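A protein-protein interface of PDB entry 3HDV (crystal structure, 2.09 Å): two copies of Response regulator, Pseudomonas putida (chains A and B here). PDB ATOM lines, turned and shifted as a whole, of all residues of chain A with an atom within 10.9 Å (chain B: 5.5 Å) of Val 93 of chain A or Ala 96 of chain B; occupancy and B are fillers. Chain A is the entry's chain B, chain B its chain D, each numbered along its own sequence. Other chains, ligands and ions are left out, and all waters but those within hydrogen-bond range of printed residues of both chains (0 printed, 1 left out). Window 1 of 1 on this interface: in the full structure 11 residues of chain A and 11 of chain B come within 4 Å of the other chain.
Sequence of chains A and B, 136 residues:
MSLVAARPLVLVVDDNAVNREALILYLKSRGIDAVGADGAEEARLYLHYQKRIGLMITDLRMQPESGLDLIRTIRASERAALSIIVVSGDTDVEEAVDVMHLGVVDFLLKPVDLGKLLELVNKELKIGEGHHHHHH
A ring nitrogen (NE2) of His 101 of chain B is in hydrogen-bond range of the side-chain carboxylate (OD1) of Asp 106 of chain A, at 2.7 Å.
The side-chain carboxylate (OD2) of Asp 92 of chain B sits close to the backbone NH (N) of Glu 94 of chain B (3.4 Å).
N of Glu 95 of chain A lies within hydrogen-bond range of OD1 of Asp 92 of chain A (2.9 Å).
OD2 of Asp 92 of chain B lies within hydrogen-bond range of N of Glu 95 of chain B, at 2.9 Å.
OD1 of Asp 92 of chain A is in hydrogen-bond range of N of Glu 94 of chain A.
Among the printed residues, merely in contact across the chains: Met 100 of chain A with Met 100 of chain B (3.5 Å), Val 93 of chain A with Asp 92 of chain B (3.5 Å), Asp 92 of chain A with Val 93 of chain B (3.5 Å), Met 100 of chain A with His 101 of chain B (3.6 Å), Met 100 of chain A with Val 97 of chain B (3.6 Å), His 101 of chain A with Met 100 of chain B (3.6 Å), Asp 106 of chain A with Val 97 of chain B (3.6 Å), Val 93 of chain A with Val 93 of chain B (3.7 Å), Phe 107 of chain A with Val 97 of chain B (3.7 Å), Glu 94 of chain A with Leu 109 of chain B (3.7 Å), Leu 109 of chain A with Glu 94 of chain B (3.7 Å), Val 97 of chain A with Met 100 of chain B (3.7 Å), Val 97 of chain A with Phe 107 of chain B (3.8 Å), Leu 109 of chain A with Val 93 of chain B (3.8 Å), Phe 107 of chain A with Val 93 of chain B (3.8 Å), Val 93 of chain A with Ala 96 of chain B (3.9 Å), Val 93 of chain A with Phe 107 of chain B (3.9 Å), Val 93 of chain A with Leu 109 of chain B (3.98 Å) and Ala 96 of chain A with Val 93 of chain B (3.98 Å).
Thr 91 of chain A touches none of the printed residues of chain B.
Val 93 of chain A touches just these residues of chain B: Asp 92, Val 93, Ala 96, Phe 107 and Leu 109.
Printed residues of chain B within 4 Å of Ala 96 of chain A: Val 93.
Of the printed residues of chain B, Leu 109 of chain A touches Val 93 and Glu 94.
No residue of chain A comes within 4 Å of Thr 91 of chain B.
Of chain A, only Val 93 comes within 4 Å of Asp 92 of chain B.
Of the printed residues of chain A, Val 93 of chain B touches Asp 92 (3.5 Å), Val 93 (3.7 Å), Ala 96 (3.98 Å), Phe 107 (3.8 Å) and Leu 109 (3.8 Å).
No residue of chain A comes within 4 Å of Glu 95 of chain B.
Of chain A, only Val 93 (3.9 Å) comes within 4 Å of Ala 96 of chain B.
Printed residues of chain A within 4 Å of Val 97 of chain B: Met 100 (3.6 Å), Asp 106 (3.6 Å) and Phe 107 (3.7 Å).
No residue of chain A comes within 4 Å of Asp 98 of chain B.
No residue of chain A comes within 4 Å of Val 99 of chain B.
Of chain A, only Val 97 (3.7 Å), Met 100 (3.5 Å) and His 101 (3.6 Å) come within 4 Å of Met 100 of chain B.
Of the 13 printed residues of chain B, 9 touch a printed residue of chain A.
Hydrophobic or aromatic side chains of chain B within 4 Å of the printed part of chain A: Val 93, Ala 96, Val 97, Met 100, His 101, Phe 107 and Leu 109.
Among the printed residues, 20 pairs touch across the chains.
Among the printed residues, no Asp or Glu carboxylate lies within 4 Å of a Lys or Arg side-chain nitrogen of the other chain.
Val 93 of chain A touches its own counterpart, Val 93 of chain B.
Val 93 of chain A touches Ala 96 of chain B, and with the chains exchanged Ala 96 of chain A touches Val 93 of chain B.
Val 93 of chain A touches Phe 107 of chain B, and with the chains exchanged Phe 107 of chain A touches Val 93 of chain B.
Glu 94 of chain A touches Leu 109 of chain B, and with the chains exchanged Leu 109 of chain A touches Glu 94 of chain B.
13 positions are printed for both chains.
Of the 20 pairs that touch across the chains among the printed residues, 18 have their exchanged pair printed and touching as well.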
ATOM      1  N   LEU A  60       6.167   8.996   4.718  1.00  0.00           N
ATOM      2  CA  LEU A  60       7.365   9.074   3.919  1.00  0.00           C
ATOM      3  C   LEU A  60       8.193   7.799   4.109  1.00  0.00           C
ATOM      4  O   LEU A  60       8.829   7.318   3.193  1.00  0.00           O
ATOM      5  CB  LEU A  60       8.172  10.299   4.357  1.00  0.00           C
ATOM      6  CG  LEU A  60       7.563  11.656   3.935  1.00  0.00           C
ATOM      7  CD1 LEU A  60       8.590  12.705   4.311  1.00  0.00           C
ATOM      8  CD2 LEU A  60       7.190  11.759   2.413  1.00  0.00           C
ATOM      9  N   ARG A  61       8.136   7.266   5.320  1.00  0.00           N
ATOM     10  CA  ARG A  61       8.910   6.124   5.770  1.00  0.00           C
ATOM     11  C   ARG A  61       8.190   4.796   5.416  1.00  0.00           C
ATOM     12  O   ARG A  61       7.372   4.281   6.176  1.00  0.00           O
ATOM     13  CB  ARG A  61       9.029   6.323   7.276  1.00  0.00           C
ATOM     14  CG  ARG A  61      10.403   6.192   7.884  1.00  0.00           C
ATOM     15  CD  ARG A  61      11.522   7.153   7.467  1.00  0.00           C
ATOM     16  NE  ARG A  61      11.832   7.246   6.034  1.00  0.00           N
ATOM     17  CZ  ARG A  61      11.915   8.414   5.416  1.00  0.00           C
ATOM     18  NH1 ARG A  61      11.698   9.547   6.112  1.00  0.00           N
ATOM     19  NH2 ARG A  61      12.192   8.469   4.141  1.00  0.00           N
ATOM     20  N   LEU A  68       8.408   9.791  -0.510  1.00  0.00           N
ATOM     21  CA  LEU A  68       8.923  10.809  -1.416  1.00  0.00           C
ATOM     22  C   LEU A  68       8.931  10.307  -2.894  1.00  0.00           C
ATOM     23  O   LEU A  68       8.524  11.030  -3.803  1.00  0.00           O
ATOM     24  CB  LEU A  68      10.311  11.287  -1.001  1.00  0.00           C
ATOM     25  CG  LEU A  68      11.155  12.126  -1.928  1.00  0.00           C
ATOM     26  CD1 LEU A  68      10.450  13.365  -2.372  1.00  0.00           C
ATOM     27  CD2 LEU A  68      12.527  12.448  -1.280  1.00  0.00           C
ATOM     28  N   SER A  88       4.302  12.204   8.508  1.00  0.00           N
ATOM     29  CA  SER A  88       5.581  11.492   8.507  1.00  0.00           C
ATOM     30  C   SER A  88       6.149  11.022   9.842  1.00  0.00           C
ATOM     31  O   SER A  88       6.123  11.772  10.855  1.00  0.00           O
ATOM     32  CB  SER A  88       6.616  12.405   7.878  1.00  0.00           C
ATOM     33  OG  SER A  88       7.814  11.709   7.689  1.00  0.00           O
ATOM     34  N   GLY A  89       6.703   9.802   9.823  1.00  0.00           N
ATOM     35  CA  GLY A  89       7.650   9.372  10.851  1.00  0.00           C
ATOM     36  C   GLY A  89       8.975  10.123  10.740  1.00  0.00           C
ATOM     37  O   GLY A  89       9.026  11.199  10.155  1.00  0.00           O
ATOM     38  N   ASP A  90      10.055   9.553  11.268  1.00  0.00           N
ATOM     39  CA  ASP A  90      11.392  10.195  11.226  1.00  0.00           C
ATOM     40  C   ASP A  90      11.760  10.735   9.839  1.00  0.00           C
ATOM     41  O   ASP A  90      11.697  10.008   8.821  1.00  0.00           O
ATOM     42  CB  ASP A  90      12.494   9.201  11.655  1.00  0.00           C
ATOM     43  CG  ASP A  90      12.338   8.709  13.117  1.00  0.00           C
ATOM     44  OD1 ASP A  90      11.565   9.313  13.937  1.00  0.00           O
ATOM     45  OD2 ASP A  90      12.988   7.678  13.432  1.00  0.00           O
ATOM     46  N   THR A  91      12.129  12.005   9.792  1.00  0.00           N
ATOM     47  CA  THR A  91      12.457  12.644   8.521  1.00  0.00           C
ATOM     48  C   THR A  91      13.511  13.710   8.881  1.00  0.00           C
ATOM     49  O   THR A  91      14.101  13.628   9.960  1.00  0.00           O
ATOM     50  CB  THR A  91      11.178  13.227   7.797  1.00  0.00           C
ATOM     51  OG1 THR A  91      11.562  13.987   6.633  1.00  0.00           O
ATOM     52  CG2 THR A  91      10.346  14.152   8.720  1.00  0.00           C
ATOM     53  N   ASP A  92      13.746  14.695   8.032  1.00  0.00           N
ATOM     54  CA  ASP A  92      14.761  15.701   8.340  1.00  0.00           C
ATOM     55  C   ASP A  92      14.462  16.851   7.425  1.00  0.00           C
ATOM     56  O   ASP A  92      13.570  16.744   6.580  1.00  0.00           O
ATOM     57  CB  ASP A  92      16.169  15.176   8.070  1.00  0.00           C
ATOM     58  CG  ASP A  92      16.294  14.535   6.671  1.00  0.00           C
ATOM     59  OD1 ASP A  92      16.112  15.222   5.676  1.00  0.00           O
ATOM     60  OD2 ASP A  92      16.570  13.321   6.564  1.00  0.00           O
ATOM     61  N   VAL A  93      15.188  17.946   7.622  1.00  0.00           N
ATOM     62  CA  VAL A  93      14.913  19.173   6.948  1.00  0.00           C
ATOM     63  C   VAL A  93      15.059  19.051   5.455  1.00  0.00           C
ATOM     64  O   VAL A  93      14.202  19.515   4.738  1.00  0.00           O
ATOM     65  CB  VAL A  93      15.744  20.354   7.521  1.00  0.00           C
ATOM     66  CG1 VAL A  93      15.635  21.584   6.613  1.00  0.00           C
ATOM     67  CG2 VAL A  93      15.266  20.660   8.948  1.00  0.00           C
ATOM     68  N   GLU A  94      16.127  18.414   4.966  1.00  0.00           N
ATOM     69  CA  GLU A  94      16.327  18.316   3.497  1.00  0.00           C
ATOM     70  C   GLU A  94      15.183  17.591   2.823  1.00  0.00           C
ATOM     71  O   GLU A  94      14.682  18.028   1.790  1.00  0.00           O
ATOM     72  CB  GLU A  94      17.698  17.670   3.164  1.00  0.00           C
ATOM     73  CG  GLU A  94      18.821  18.670   3.548  1.00  0.00           C
ATOM     74  CD  GLU A  94      20.229  18.340   3.034  1.00  0.00           C
ATOM     75  OE1 GLU A  94      20.525  17.129   2.786  1.00  0.00           O
ATOM     76  OE2 GLU A  94      21.042  19.348   2.921  1.00  0.00           O
ATOM     77  N   GLU A  95      14.776  16.470   3.410  1.00  0.00           N
ATOM     78  CA  GLU A  95      13.662  15.723   2.863  1.00  0.00           C
ATOM     79  C   GLU A  95      12.352  16.569   2.904  1.00  0.00           C
ATOM     80  O   GLU A  95      11.577  16.591   1.935  1.00  0.00           O
ATOM     81  CB  GLU A  95      13.482  14.400   3.610  1.00  0.00           C
ATOM     82  CG  GLU A  95      12.357  13.539   3.002  1.00  0.00           C
ATOM     83  CD  GLU A  95      12.248  12.203   3.626  1.00  0.00           C
ATOM     84  OE1 GLU A  95      12.270  12.095   4.872  1.00  0.00           O
ATOM     85  OE2 GLU A  95      12.101  11.230   2.873  1.00  0.00           O
ATOM     86  N   ALA A  96      12.106  17.255   4.023  1.00  0.00           N
ATOM     87  CA  ALA A  96      10.888  18.094   4.129  1.00  0.00           C
ATOM     88  C   ALA A  96      10.855  19.175   3.051  1.00  0.00           C
ATOM     89  O   ALA A  96       9.817  19.430   2.433  1.00  0.00           O
ATOM     90  CB  ALA A  96      10.752  18.693   5.553  1.00  0.00           C
ATOM     91  N   VAL A  97      12.020  19.767   2.774  1.00  0.00           N
ATOM     92  CA  VAL A  97      12.098  20.783   1.747  1.00  0.00           C
ATOM     93  C   VAL A  97      11.851  20.162   0.355  1.00  0.00           C
ATOM     94  O   VAL A  97      11.129  20.734  -0.440  1.00  0.00           O
ATOM     95  CB  VAL A  97      13.443  21.559   1.828  1.00  0.00           C
ATOM     96  CG1 VAL A  97      13.669  22.361   0.544  1.00  0.00           C
ATOM     97  CG2 VAL A  97      13.484  22.471   3.130  1.00  0.00           C
ATOM     98  N   ASP A  98      12.484  18.997   0.067  1.00  0.00           N
ATOM     99  CA  ASP A  98      12.194  18.247  -1.174  1.00  0.00           C
ATOM    100  C   ASP A  98      10.697  17.970  -1.336  1.00  0.00           C
ATOM    101  O   ASP A  98      10.127  18.224  -2.391  1.00  0.00           O
ATOM    102  CB  ASP A  98      12.929  16.891  -1.175  1.00  0.00           C
ATOM    103  CG  ASP A  98      14.420  17.029  -1.446  1.00  0.00           C
ATOM    104  OD1 ASP A  98      14.841  18.036  -2.069  1.00  0.00           O
ATOM    105  OD2 ASP A  98      15.175  16.123  -1.033  1.00  0.00           O
ATOM    106  N   VAL A  99      10.067  17.438  -0.302  1.00  0.00           N
ATOM    107  CA  VAL A  99       8.617  17.185  -0.343  1.00  0.00           C
ATOM    108  C   VAL A  99       7.801  18.461  -0.574  1.00  0.00           C
ATOM    109  O   VAL A  99       6.872  18.503  -1.439  1.00  0.00           O
ATOM    110  CB  VAL A  99       8.141  16.388   0.884  1.00  0.00           C
ATOM    111  CG1 VAL A  99       6.576  16.233   0.901  1.00  0.00           C
ATOM    112  CG2 VAL A  99       8.812  15.019   0.868  1.00  0.00           C
ATOM    113  N   MET A 100       8.168  19.527   0.132  1.00  0.00           N
ATOM    114  CA  MET A 100       7.452  20.790  -0.044  1.00  0.00           C
ATOM    115  C   MET A 100       7.595  21.364  -1.484  1.00  0.00           C
ATOM    116  O   MET A 100       6.652  21.945  -2.015  1.00  0.00           O
ATOM    117  CB  MET A 100       7.814  21.806   1.067  1.00  0.00           C
ATOM    118  CG  MET A 100       7.381  21.380   2.505  1.00  0.00           C
ATOM    119  SD  MET A 100       5.386  21.490   2.628  1.00  0.00           S
ATOM    120  CE  MET A 100       5.297  23.472   2.689  1.00  0.00           C
ATOM    121  N   HIS A 101       8.756  21.201  -2.113  1.00  0.00           N
ATOM    122  CA  HIS A 101       8.886  21.594  -3.529  1.00  0.00           C
ATOM    123  C   HIS A 101       7.985  20.807  -4.453  1.00  0.00           C
ATOM    124  O   HIS A 101       7.656  21.295  -5.548  1.00  0.00           O
ATOM    125  CB  HIS A 101      10.317  21.436  -4.047  1.00  0.00           C
ATOM    126  CG  HIS A 101      11.274  22.486  -3.572  1.00  0.00           C
ATOM    127  ND1 HIS A 101      11.148  23.819  -3.910  1.00  0.00           N
ATOM    128  CD2 HIS A 101      12.447  22.378  -2.895  1.00  0.00           C
ATOM    129  CE1 HIS A 101      12.180  24.493  -3.427  1.00  0.00           C
ATOM    130  NE2 HIS A 101      13.000  23.636  -2.836  1.00  0.00           N
ATOM    131  N   VAL A 104       2.974  19.523  -1.786  1.00  0.00           N
ATOM    132  CA  VAL A 104       1.989  18.870  -0.924  1.00  0.00           C
ATOM    133  C   VAL A 104       1.068  19.907  -0.265  1.00  0.00           C
ATOM    134  O   VAL A 104       1.438  21.047  -0.121  1.00  0.00           O
ATOM    135  CB  VAL A 104       2.650  17.885   0.076  1.00  0.00           C
ATOM    136  CG1 VAL A 104       3.444  16.834  -0.674  1.00  0.00           C
ATOM    137  CG2 VAL A 104       3.551  18.630   1.118  1.00  0.00           C
ATOM    138  N   ASP A 106       0.079  19.809   2.981  1.00  0.00           N
ATOM    139  CA  ASP A 106       0.826  20.125   4.198  1.00  0.00           C
ATOM    140  C   ASP A 106       1.691  18.937   4.542  1.00  0.00           C
ATOM    141  O   ASP A 106       1.541  17.869   3.917  1.00  0.00           O
ATOM    142  CB  ASP A 106      -0.125  20.409   5.374  1.00  0.00           C
ATOM    143  CG  ASP A 106       0.466  21.391   6.397  1.00  0.00           C
ATOM    144  OD1 ASP A 106       1.719  21.605   6.506  1.00  0.00           O
ATOM    145  OD2 ASP A 106      -0.361  21.993   7.094  1.00  0.00           O
ATOM    146  N   PHE A 107       2.558  19.113   5.560  1.00  0.00           N
ATOM    147  CA  PHE A 107       3.550  18.116   5.944  1.00  0.00           C
ATOM    148  C   PHE A 107       3.432  18.109   7.458  1.00  0.00           C
ATOM    149  O   PHE A 107       3.867  19.051   8.110  1.00  0.00           O
ATOM    150  CB  PHE A 107       4.930  18.589   5.455  1.00  0.00           C
ATOM    151  CG  PHE A 107       6.074  17.609   5.653  1.00  0.00           C
ATOM    152  CD1 PHE A 107       6.773  17.126   4.554  1.00  0.00           C
ATOM    153  CD2 PHE A 107       6.511  17.238   6.935  1.00  0.00           C
ATOM    154  CE1 PHE A 107       7.864  16.231   4.695  1.00  0.00           C
ATOM    155  CE2 PHE A 107       7.606  16.329   7.104  1.00  0.00           C
ATOM    156  CZ  PHE A 107       8.281  15.835   5.983  1.00  0.00           C
ATOM    157  N   LEU A 108       2.853  17.054   8.017  1.00  0.00           N
ATOM    158  CA  LEU A 108       2.666  16.938   9.449  1.00  0.00           C
ATOM    159  C   LEU A 108       3.588  15.890  10.032  1.00  0.00           C
ATOM    160  O   LEU A 108       3.822  14.864   9.410  1.00  0.00           O
ATOM    161  CB  LEU A 108       1.225  16.515   9.745  1.00  0.00           C
ATOM    162  CG  LEU A 108       0.118  17.563   9.845  1.00  0.00           C
ATOM    163  CD1 LEU A 108       0.211  18.602   8.813  1.00  0.00           C
ATOM    164  CD2 LEU A 108      -1.315  16.943   9.903  1.00  0.00           C
ATOM    165  N   LEU A 109       4.048  16.089  11.259  1.00  0.00           N
ATOM    166  CA  LEU A 109       4.850  15.055  11.928  1.00  0.00           C
ATOM    167  C   LEU A 109       3.998  14.192  12.840  1.00  0.00           C
ATOM    168  O   LEU A 109       3.061  14.677  13.479  1.00  0.00           O
ATOM    169  CB  LEU A 109       6.057  15.667  12.676  1.00  0.00           C
ATOM    170  CG  LEU A 109       7.107  16.469  11.869  1.00  0.00           C
ATOM    171  CD1 LEU A 109       8.104  17.161  12.837  1.00  0.00           C
ATOM    172  CD2 LEU A 109       7.860  15.540  10.951  1.00  0.00           C
ATOM    173  N   LYS A 116      -5.943  19.157  13.619  1.00  0.00           N
ATOM    174  CA  LYS A 116      -5.351  19.874  12.468  1.00  0.00           C
ATOM    175  C   LYS A 116      -5.490  19.079  11.161  1.00  0.00           C
ATOM    176  O   LYS A 116      -5.809  19.644  10.088  1.00  0.00           O
ATOM    177  CB  LYS A 116      -3.876  20.171  12.708  1.00  0.00           C
ATOM    178  CG  LYS A 116      -3.142  20.904  11.548  1.00  0.00           C
ATOM    179  CD  LYS A 116      -1.611  20.819  11.761  1.00  0.00           C
ATOM    180  CE  LYS A 116      -0.817  21.876  10.929  1.00  0.00           C
ATOM    181  NZ  LYS A 116       0.672  21.877  11.309  1.00  0.00           N
ATOM    182  N   THR B  91      17.926  24.978  12.336  1.00  0.00           N
ATOM    183  CA  THR B  91      16.478  24.942  12.057  1.00  0.00           C
ATOM    184  C   THR B  91      15.908  23.565  12.365  1.00  0.00           C
ATOM    185  O   THR B  91      16.610  22.710  12.925  1.00  0.00           O
ATOM    186  CB  THR B  91      16.129  25.441  10.599  1.00  0.00           C
ATOM    187  OG1 THR B  91      14.701  25.445  10.380  1.00  0.00           O
ATOM    188  CG2 THR B  91      16.814  24.597   9.546  1.00  0.00           C
ATOM    189  N   ASP B  92      14.638  23.353  12.007  1.00  0.00           N
ATOM    190  CA  ASP B  92      14.007  22.045  12.211  1.00  0.00           C
ATOM    191  C   ASP B  92      12.887  21.840  11.211  1.00  0.00           C
ATOM    192  O   ASP B  92      12.542  22.738  10.478  1.00  0.00           O
ATOM    193  CB  ASP B  92      13.516  21.847  13.658  1.00  0.00           C
ATOM    194  CG  ASP B  92      12.514  22.920  14.112  1.00  0.00           C
ATOM    195  OD1 ASP B  92      12.682  23.421  15.247  1.00  0.00           O
ATOM    196  OD2 ASP B  92      11.573  23.280  13.384  1.00  0.00           O
ATOM    197  N   VAL B  93      12.356  20.629  11.175  1.00  0.00           N
ATOM    198  CA  VAL B  93      11.379  20.242  10.162  1.00  0.00           C
ATOM    199  C   VAL B  93      10.136  21.136  10.170  1.00  0.00           C
ATOM    200  O   VAL B  93       9.736  21.590   9.129  1.00  0.00           O
ATOM    201  CB  VAL B  93      11.005  18.751  10.305  1.00  0.00           C
ATOM    202  CG1 VAL B  93       9.782  18.425   9.408  1.00  0.00           C
ATOM    203  CG2 VAL B  93      12.240  17.904   9.912  1.00  0.00           C
ATOM    204  N   GLU B  94       9.560  21.394  11.354  1.00  0.00           N
ATOM    205  CA  GLU B  94       8.338  22.210  11.440  1.00  0.00           C
ATOM    206  C   GLU B  94       8.560  23.654  10.976  1.00  0.00           C
ATOM    207  O   GLU B  94       7.721  24.227  10.310  1.00  0.00           O
ATOM    208  CB  GLU B  94       7.730  22.129  12.845  1.00  0.00           C
ATOM    209  CG  GLU B  94       7.110  20.728  13.068  1.00  0.00           C
ATOM    210  CD  GLU B  94       6.380  20.579  14.405  1.00  0.00           C
ATOM    211  OE1 GLU B  94       6.449  21.549  15.201  1.00  0.00           O
ATOM    212  OE2 GLU B  94       5.712  19.504  14.636  1.00  0.00           O
ATOM    213  N   GLU B  95       9.737  24.205  11.269  1.00  0.00           N
ATOM    214  CA  GLU B  95      10.063  25.566  10.809  1.00  0.00           C
ATOM    215  C   GLU B  95      10.274  25.605   9.302  1.00  0.00           C
ATOM    216  O   GLU B  95       9.761  26.505   8.608  1.00  0.00           O
ATOM    217  CB  GLU B  95      11.342  26.115  11.507  1.00  0.00           C
ATOM    218  CG  GLU B  95      11.670  27.549  11.066  1.00  0.00           C
ATOM    219  CD  GLU B  95      12.781  28.185  11.920  1.00  0.00           C
ATOM    220  OE1 GLU B  95      13.469  27.413  12.617  1.00  0.00           O
ATOM    221  OE2 GLU B  95      12.929  29.440  11.918  1.00  0.00           O
ATOM    222  N   ALA B  96      11.016  24.619   8.782  1.00  0.00           N
ATOM    223  CA  ALA B  96      11.220  24.551   7.336  1.00  0.00           C
ATOM    224  C   ALA B  96       9.873  24.475   6.587  1.00  0.00           C
ATOM    225  O   ALA B  96       9.665  25.131   5.578  1.00  0.00           O
ATOM    226  CB  ALA B  96      12.142  23.322   6.993  1.00  0.00           C
ATOM    227  N   VAL B  97       8.968  23.637   7.061  1.00  0.00           N
ATOM    228  CA  VAL B  97       7.605  23.524   6.460  1.00  0.00           C
ATOM    229  C   VAL B  97       6.845  24.864   6.602  1.00  0.00           C
ATOM    230  O   VAL B  97       6.299  25.340   5.624  1.00  0.00           O
ATOM    231  CB  VAL B  97       6.827  22.352   7.113  1.00  0.00           C
ATOM    232  CG1 VAL B  97       5.235  22.445   6.868  1.00  0.00           C
ATOM    233  CG2 VAL B  97       7.439  21.015   6.694  1.00  0.00           C
ATOM    234  N   ASP B  98       6.840  25.478   7.800  1.00  0.00           N
ATOM    235  CA  ASP B  98       6.262  26.836   7.986  1.00  0.00           C
ATOM    236  C   ASP B  98       6.777  27.820   6.926  1.00  0.00           C
ATOM    237  O   ASP B  98       6.039  28.552   6.271  1.00  0.00           O
ATOM    238  CB  ASP B  98       6.668  27.396   9.367  1.00  0.00           C
ATOM    239  CG  ASP B  98       5.809  26.866  10.501  1.00  0.00           C
ATOM    240  OD1 ASP B  98       4.704  26.344  10.255  1.00  0.00           O
ATOM    241  OD2 ASP B  98       6.238  26.997  11.652  1.00  0.00           O
ATOM    242  N   VAL B  99       8.081  27.830   6.751  1.00  0.00           N
ATOM    243  CA  VAL B  99       8.705  28.749   5.792  1.00  0.00           C
ATOM    244  C   VAL B  99       8.355  28.373   4.375  1.00  0.00           C
ATOM    245  O   VAL B  99       8.088  29.254   3.558  1.00  0.00           O
ATOM    246  CB  VAL B  99      10.266  28.722   5.906  1.00  0.00           C
ATOM    247  CG1 VAL B  99      10.910  29.464   4.701  1.00  0.00           C
ATOM    248  CG2 VAL B  99      10.701  29.302   7.194  1.00  0.00           C
ATOM    249  N   MET B 100       8.389  27.069   4.068  1.00  0.00           N
ATOM    250  CA  MET B 100       8.043  26.616   2.674  1.00  0.00           C
ATOM    251  C   MET B 100       6.580  26.979   2.318  1.00  0.00           C
ATOM    252  O   MET B 100       6.258  27.299   1.140  1.00  0.00           O
ATOM    253  CB  MET B 100       8.349  25.113   2.482  1.00  0.00           C
ATOM    254  CG  MET B 100       9.838  24.776   2.424  1.00  0.00           C
ATOM    255  SD  MET B 100      10.691  25.530   0.876  1.00  0.00           S
ATOM    256  CE  MET B 100       9.954  24.292  -0.517  1.00  0.00           C
ATOM    257  N   HIS B 101       5.684  26.976   3.319  1.00  0.00           N
ATOM    258  CA  HIS B 101       4.284  27.481   3.059  1.00  0.00           C
ATOM    259  C   HIS B 101       4.191  28.966   2.607  1.00  0.00           C
ATOM    260  O   HIS B 101       3.185  29.420   1.981  1.00  0.00           O
ATOM    261  CB  HIS B 101       3.380  27.290   4.251  1.00  0.00           C
ATOM    262  CG  HIS B 101       2.882  25.878   4.430  1.00  0.00           C
ATOM    263  ND1 HIS B 101       2.075  25.255   3.511  1.00  0.00           N
ATOM    264  CD2 HIS B 101       3.016  25.011   5.457  1.00  0.00           C
ATOM    265  CE1 HIS B 101       1.745  24.057   3.949  1.00  0.00           C
ATOM    266  NE2 HIS B 101       2.304  23.884   5.133  1.00  0.00           N
ATOM    267  N   PHE B 107      15.278  26.769   0.130  1.00  0.00           N
ATOM    268  CA  PHE B 107      15.569  26.723   1.506  1.00  0.00           C
ATOM    269  C   PHE B 107      16.818  25.826   1.514  1.00  0.00           C
ATOM    270  O   PHE B 107      16.751  24.642   1.176  1.00  0.00           O
ATOM    271  CB  PHE B 107      14.380  26.082   2.213  1.00  0.00           C
ATOM    272  CG  PHE B 107      14.460  26.105   3.694  1.00  0.00           C
ATOM    273  CD1 PHE B 107      13.511  26.825   4.432  1.00  0.00           C
ATOM    274  CD2 PHE B 107      15.465  25.403   4.380  1.00  0.00           C
ATOM    275  CE1 PHE B 107      13.546  26.844   5.842  1.00  0.00           C
ATOM    276  CE2 PHE B 107      15.523  25.418   5.783  1.00  0.00           C
ATOM    277  CZ  PHE B 107      14.529  26.155   6.522  1.00  0.00           C
ATOM    278  N   LEU B 109      20.406  24.483   3.522  1.00  0.00           N
ATOM    279  CA  LEU B 109      21.105  24.381   4.805  1.00  0.00           C
ATOM    280  C   LEU B 109      22.539  24.859   4.734  1.00  0.00           C
ATOM    281  O   LEU B 109      23.220  24.663   3.739  1.00  0.00           O
ATOM    282  CB  LEU B 109      21.072  22.943   5.339  1.00  0.00           C
ATOM    283  CG  LEU B 109      19.782  22.327   5.890  1.00  0.00           C
ATOM    284  CD1 LEU B 109      20.079  20.860   6.257  1.00  0.00           C
ATOM    285  CD2 LEU B 109      19.257  23.143   7.136  1.00  0.00           C
